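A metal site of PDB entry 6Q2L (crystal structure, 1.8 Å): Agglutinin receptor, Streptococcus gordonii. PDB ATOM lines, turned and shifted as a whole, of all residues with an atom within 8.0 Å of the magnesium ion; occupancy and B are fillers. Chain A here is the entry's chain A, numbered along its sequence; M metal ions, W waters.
The side-chain hydroxyl of Ser 191 sits close to the side-chain carboxylate of Asp 253.
The backbone NH of Ser 191 is in hydrogen-bond range of the backbone carbonyl oxygen of Gly 263 (3.4 Å).
ND2 of Asn 193 lies within hydrogen-bond range of OD2 of Asp 253, at 3.0 Å.
The magnesium ion is bound by the side-chain hydroxyl (OG) of Ser 191 (2.2 Å), water W3 (2.2 Å), the backbone carbonyl oxygen (O) of Ser 191 (2.2 Å), the side-chain amide oxygen (OD1) of Asn 193 (2.3 Å) and the side-chain carboxylate (OE1) of Glu 207 (2.3 Å).
The magnesium ion has five donor atoms within binding distance.
Within 4 Å of the magnesium ion: Ser 191, Asn 193 and Glu 207.
Water W2 bridges the side-chain carboxylate of Glu 207 (2.8 Å) and the backbone NH of Trp 287 (3.3 Å).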
ATOM      1  N   TRP A 156     -31.870  -5.791   6.103  1.00  0.00           N
ATOM      2  CA  TRP A 156     -32.388  -7.143   6.010  1.00  0.00           C
ATOM      3  C   TRP A 156     -32.246  -7.557   4.569  1.00  0.00           C
ATOM      4  O   TRP A 156     -32.465  -6.728   3.675  1.00  0.00           O
ATOM      5  CB  TRP A 156     -33.867  -7.221   6.365  1.00  0.00           C
ATOM      6  CG  TRP A 156     -34.158  -7.129   7.823  1.00  0.00           C
ATOM      7  CD1 TRP A 156     -34.128  -6.001   8.591  1.00  0.00           C
ATOM      8  CD2 TRP A 156     -34.568  -8.202   8.685  1.00  0.00           C
ATOM      9  NE1 TRP A 156     -34.467  -6.308   9.884  1.00  0.00           N
ATOM     10  CE2 TRP A 156     -34.753  -7.640   9.971  1.00  0.00           C
ATOM     11  CE3 TRP A 156     -34.764  -9.574   8.497  1.00  0.00           C
ATOM     12  CZ2 TRP A 156     -35.162  -8.423  11.081  1.00  0.00           C
ATOM     13  CZ3 TRP A 156     -35.157 -10.355   9.608  1.00  0.00           C
ATOM     14  CH2 TRP A 156     -35.348  -9.775  10.871  1.00  0.00           C
ATOM     15  N   SER A 190     -22.454 -10.007  14.303  1.00  0.00           N
ATOM     16  CA  SER A 190     -23.293 -10.666  15.292  1.00  0.00           C
ATOM     17  C   SER A 190     -24.334 -11.562  14.662  1.00  0.00           C
ATOM     18  O   SER A 190     -24.576 -11.532  13.433  1.00  0.00           O
ATOM     19  CB  SER A 190     -24.036  -9.602  16.099  1.00  0.00           C
ATOM     20  OG  SER A 190     -24.775  -8.777  15.218  1.00  0.00           O
ATOM     21  N   SER A 191     -25.007 -12.303  15.539  1.00  0.00           N
ATOM     22  CA  SER A 191     -26.183 -13.115  15.178  1.00  0.00           C
ATOM     23  C   SER A 191     -25.899 -13.942  13.921  1.00  0.00           C
ATOM     24  O   SER A 191     -26.647 -13.932  13.060  1.00  0.00           O
ATOM     25  CB  SER A 191     -27.398 -12.231  15.040  1.00  0.00           C
ATOM     26  OG  SER A 191     -28.567 -12.930  14.712  1.00  0.00           O
ATOM     27  N   LEU A 192     -24.777 -14.624  13.863  1.00  0.00           N
ATOM     28  CA  LEU A 192     -24.423 -15.436  12.716  1.00  0.00           C
ATOM     29  C   LEU A 192     -24.993 -16.821  12.960  1.00  0.00           C
ATOM     30  O   LEU A 192     -24.268 -17.776  13.292  1.00  0.00           O
ATOM     31  CB  LEU A 192     -22.924 -15.446  12.447  1.00  0.00           C
ATOM     32  CG  LEU A 192     -22.389 -14.098  11.939  1.00  0.00           C
ATOM     33  CD1 LEU A 192     -20.877 -14.131  11.924  1.00  0.00           C
ATOM     34  CD2 LEU A 192     -22.927 -13.718  10.554  1.00  0.00           C
ATOM     35  N   ASN A 193     -26.300 -16.910  12.756  1.00  0.00           N
ATOM     36  CA  ASN A 193     -27.055 -18.126  13.071  1.00  0.00           C
ATOM     37  C   ASN A 193     -26.721 -19.299  12.154  1.00  0.00           C
ATOM     38  O   ASN A 193     -26.540 -19.150  10.932  1.00  0.00           O
ATOM     39  CB  ASN A 193     -28.549 -17.870  12.976  1.00  0.00           C
ATOM     40  CG  ASN A 193     -29.011 -16.729  13.867  1.00  0.00           C
ATOM     41  OD1 ASN A 193     -29.118 -15.610  13.402  1.00  0.00           O
ATOM     42  ND2 ASN A 193     -29.201 -17.000  15.151  1.00  0.00           N
ATOM     43  N   ARG A 194     -26.649 -20.475  12.754  1.00  0.00           N
ATOM     44  CA  ARG A 194     -26.660 -21.727  12.010  1.00  0.00           C
ATOM     45  C   ARG A 194     -27.590 -22.682  12.723  1.00  0.00           C
ATOM     46  O   ARG A 194     -27.510 -22.854  13.930  1.00  0.00           O
ATOM     47  CB  ARG A 194     -25.250 -22.323  11.880  1.00  0.00           C
ATOM     48  CG  ARG A 194     -25.276 -23.691  11.247  1.00  0.00           C
ATOM     49  CD  ARG A 194     -23.952 -24.095  10.618  1.00  0.00           C
ATOM     50  NE  ARG A 194     -24.116 -25.275   9.782  1.00  0.00           N
ATOM     51  CZ  ARG A 194     -23.204 -25.791   8.963  1.00  0.00           C
ATOM     52  NH1 ARG A 194     -21.990 -25.245   8.843  1.00  0.00           N
ATOM     53  NH2 ARG A 194     -23.507 -26.877   8.246  1.00  0.00           N
ATOM     54  N   ASN A 196     -30.978 -22.420  12.584  1.00  0.00           N
ATOM     55  CA  ASN A 196     -32.209 -21.727  12.979  1.00  0.00           C
ATOM     56  C   ASN A 196     -33.203 -21.613  11.806  1.00  0.00           C
ATOM     57  O   ASN A 196     -34.010 -20.688  11.758  1.00  0.00           O
ATOM     58  CB  ASN A 196     -31.832 -20.334  13.515  1.00  0.00           C
ATOM     59  CG  ASN A 196     -32.830 -19.782  14.515  1.00  0.00           C
ATOM     60  OD1 ASN A 196     -33.253 -20.473  15.463  1.00  0.00           O
ATOM     61  ND2 ASN A 196     -33.181 -18.517  14.332  1.00  0.00           N
ATOM     62  N   GLU A 207     -26.047 -18.394   8.260  1.00  0.00           N
ATOM     63  CA  GLU A 207     -25.722 -16.989   8.045  1.00  0.00           C
ATOM     64  C   GLU A 207     -24.221 -16.820   8.207  1.00  0.00           C
ATOM     65  O   GLU A 207     -23.644 -17.375   9.150  1.00  0.00           O
ATOM     66  CB  GLU A 207     -26.465 -16.110   9.026  1.00  0.00           C
ATOM     67  CG  GLU A 207     -27.969 -16.249   8.931  1.00  0.00           C
ATOM     68  CD  GLU A 207     -28.757 -15.353   9.864  1.00  0.00           C
ATOM     69  OE1 GLU A 207     -28.210 -14.449  10.583  1.00  0.00           O
ATOM     70  OE2 GLU A 207     -29.982 -15.576   9.883  1.00  0.00           O
ATOM     71  N   SER A 208     -23.599 -16.074   7.299  1.00  0.00           N
ATOM     72  CA  SER A 208     -22.148 -15.896   7.301  1.00  0.00           C
ATOM     73  C   SER A 208     -21.733 -14.494   6.873  1.00  0.00           C
ATOM     74  O   SER A 208     -22.537 -13.727   6.318  1.00  0.00           O
ATOM     75  CB  SER A 208     -21.492 -16.958   6.415  1.00  0.00           C
ATOM     76  OG  SER A 208     -21.793 -16.796   5.031  1.00  0.00           O
ATOM     77  N   THR A 249     -31.055 -20.657  20.424  1.00  0.00           N
ATOM     78  CA  THR A 249     -31.017 -19.312  19.869  1.00  0.00           C
ATOM     79  C   THR A 249     -31.570 -18.245  20.825  1.00  0.00           C
ATOM     80  O   THR A 249     -30.914 -17.227  21.113  1.00  0.00           O
ATOM     81  CB  THR A 249     -31.817 -19.244  18.562  1.00  0.00           C
ATOM     82  OG1 THR A 249     -31.304 -20.229  17.671  1.00  0.00           O
ATOM     83  CG2 THR A 249     -31.715 -17.864  17.895  1.00  0.00           C
ATOM     84  N   TRP A 252     -29.365 -16.834  23.644  1.00  0.00           N
ATOM     85  CA  TRP A 252     -28.177 -16.008  23.380  1.00  0.00           C
ATOM     86  C   TRP A 252     -28.365 -14.891  22.357  1.00  0.00           C
ATOM     87  O   TRP A 252     -27.715 -13.874  22.474  1.00  0.00           O
ATOM     88  CB  TRP A 252     -26.969 -16.878  22.962  1.00  0.00           C
ATOM     89  CG  TRP A 252     -27.101 -17.543  21.640  1.00  0.00           C
ATOM     90  CD1 TRP A 252     -27.479 -18.833  21.410  1.00  0.00           C
ATOM     91  CD2 TRP A 252     -26.802 -16.973  20.366  1.00  0.00           C
ATOM     92  NE1 TRP A 252     -27.472 -19.083  20.072  1.00  0.00           N
ATOM     93  CE2 TRP A 252     -27.070 -17.958  19.401  1.00  0.00           C
ATOM     94  CE3 TRP A 252     -26.387 -15.706  19.941  1.00  0.00           C
ATOM     95  CZ2 TRP A 252     -26.901 -17.736  18.033  1.00  0.00           C
ATOM     96  CZ3 TRP A 252     -26.242 -15.480  18.574  1.00  0.00           C
ATOM     97  CH2 TRP A 252     -26.493 -16.488  17.639  1.00  0.00           C
ATOM     98  N   ASP A 253     -29.217 -15.069  21.357  1.00  0.00           N
ATOM     99  CA  ASP A 253     -29.268 -14.149  20.248  1.00  0.00           C
ATOM    100  C   ASP A 253     -30.234 -12.972  20.508  1.00  0.00           C
ATOM    101  O   ASP A 253     -31.239 -12.823  19.834  1.00  0.00           O
ATOM    102  CB  ASP A 253     -29.639 -14.899  18.971  1.00  0.00           C
ATOM    103  CG  ASP A 253     -29.423 -14.053  17.726  1.00  0.00           C
ATOM    104  OD1 ASP A 253     -28.841 -12.957  17.844  1.00  0.00           O
ATOM    105  OD2 ASP A 253     -29.833 -14.488  16.644  1.00  0.00           O
ATOM    106  N   GLY A 263     -22.719 -16.262  19.235  1.00  0.00           N
ATOM    107  CA  GLY A 263     -22.926 -16.199  17.783  1.00  0.00           C
ATOM    108  C   GLY A 263     -22.221 -15.069  17.058  1.00  0.00           C
ATOM    109  O   GLY A 263     -22.673 -14.676  15.982  1.00  0.00           O
ATOM    110  N   SER A 283     -32.199 -19.337   4.704  1.00  0.00           N
ATOM    111  CA  SER A 283     -32.608 -18.557   5.866  1.00  0.00           C
ATOM    112  C   SER A 283     -33.922 -17.814   5.717  1.00  0.00           C
ATOM    113  O   SER A 283     -34.544 -17.472   6.721  1.00  0.00           O
ATOM    114  CB  SER A 283     -31.492 -17.568   6.262  1.00  0.00           C
ATOM    115  OG  SER A 283     -30.327 -18.263   6.624  1.00  0.00           O
ATOM    116  N   ASN A 285     -35.253 -14.835   5.631  1.00  0.00           N
ATOM    117  CA  ASN A 285     -34.933 -13.464   5.994  1.00  0.00           C
ATOM    118  C   ASN A 285     -33.653 -13.467   6.788  1.00  0.00           C
ATOM    119  O   ASN A 285     -33.414 -14.367   7.615  1.00  0.00           O
ATOM    120  CB  ASN A 285     -36.022 -12.854   6.907  1.00  0.00           C
ATOM    121  CG  ASN A 285     -37.368 -12.679   6.221  1.00  0.00           C
ATOM    122  OD1 ASN A 285     -37.481 -12.755   4.998  1.00  0.00           O
ATOM    123  ND2 ASN A 285     -38.385 -12.441   7.024  1.00  0.00           N
ATOM    124  N   ILE A 286     -32.819 -12.453   6.559  1.00  0.00           N
ATOM    125  CA  ILE A 286     -31.555 -12.292   7.308  1.00  0.00           C
ATOM    126  C   ILE A 286     -31.453 -10.831   7.706  1.00  0.00           C
ATOM    127  O   ILE A 286     -31.506  -9.951   6.849  1.00  0.00           O
ATOM    128  CB  ILE A 286     -30.317 -12.689   6.469  1.00  0.00           C
ATOM    129  CG1 ILE A 286     -30.427 -14.130   5.956  1.00  0.00           C
ATOM    130  CG2 ILE A 286     -29.022 -12.533   7.272  1.00  0.00           C
ATOM    131  CD1 ILE A 286     -31.182 -14.280   4.642  1.00  0.00           C
ATOM    132  N   TRP A 287     -31.305 -10.569   9.003  1.00  0.00           N
ATOM    133  CA  TRP A 287     -30.994  -9.250   9.519  1.00  0.00           C
ATOM    134  C   TRP A 287     -29.475  -9.137   9.682  1.00  0.00           C
ATOM    135  O   TRP A 287     -28.884  -9.869  10.465  1.00  0.00           O
ATOM    136  CB  TRP A 287     -31.694  -9.010  10.853  1.00  0.00           C
ATOM    137  CG  TRP A 287     -31.360  -7.687  11.496  1.00  0.00           C
ATOM    138  CD1 TRP A 287     -30.862  -6.573  10.879  1.00  0.00           C
ATOM    139  CD2 TRP A 287     -31.485  -7.351  12.873  1.00  0.00           C
ATOM    140  NE1 TRP A 287     -30.660  -5.579  11.798  1.00  0.00           N
ATOM    141  CE2 TRP A 287     -31.029  -6.027  13.029  1.00  0.00           C
ATOM    142  CE3 TRP A 287     -31.943  -8.043  14.004  1.00  0.00           C
ATOM    143  CZ2 TRP A 287     -31.022  -5.371  14.272  1.00  0.00           C
ATOM    144  CZ3 TRP A 287     -31.935  -7.402  15.249  1.00  0.00           C
ATOM    145  CH2 TRP A 287     -31.475  -6.075  15.367  1.00  0.00           C
ATOM    146  N   PHE A 288     -28.856  -8.230   8.920  1.00  0.00           N
ATOM    147  CA  PHE A 288     -27.409  -7.998   9.007  1.00  0.00           C
ATOM    148  C   PHE A 288     -27.167  -6.561   9.494  1.00  0.00           C
ATOM    149  O   PHE A 288     -27.284  -5.604   8.728  1.00  0.00           O
ATOM    150  CB  PHE A 288     -26.727  -8.220   7.656  1.00  0.00           C
ATOM    151  CG  PHE A 288     -25.244  -8.448   7.764  1.00  0.00           C
ATOM    152  CD1 PHE A 288     -24.362  -7.375   8.008  1.00  0.00           C
ATOM    153  CD2 PHE A 288     -24.713  -9.729   7.616  1.00  0.00           C
ATOM    154  CE1 PHE A 288     -22.995  -7.601   8.111  1.00  0.00           C
ATOM    155  CE2 PHE A 288     -23.342  -9.954   7.727  1.00  0.00           C
ATOM    156  CZ  PHE A 288     -22.485  -8.882   7.986  1.00  0.00           C
ATOM    157  N   ALA A 289     -26.842  -6.453  10.778  1.00  0.00           N
ATOM    158  CA  ALA A 289     -26.492  -5.195  11.401  1.00  0.00           C
ATOM    159  C   ALA A 289     -24.979  -5.004  11.343  1.00  0.00           C
ATOM    160  O   ALA A 289     -24.210  -5.939  11.624  1.00  0.00           O
ATOM    161  CB  ALA A 289     -26.984  -5.170  12.845  1.00  0.00           C
HETATM  162 MG    MG M   1     -28.779 -13.487  12.624  1.00  0.00          MG
HETATM  163  O   HOH W   1     -31.664 -13.920  13.403  1.00  0.00           O
HETATM  164  O   HOH W   2     -31.222 -13.289  10.806  1.00  0.00           O
HETATM  165  O   HOH W   3     -28.138 -11.538  11.908  1.00  0.00           O
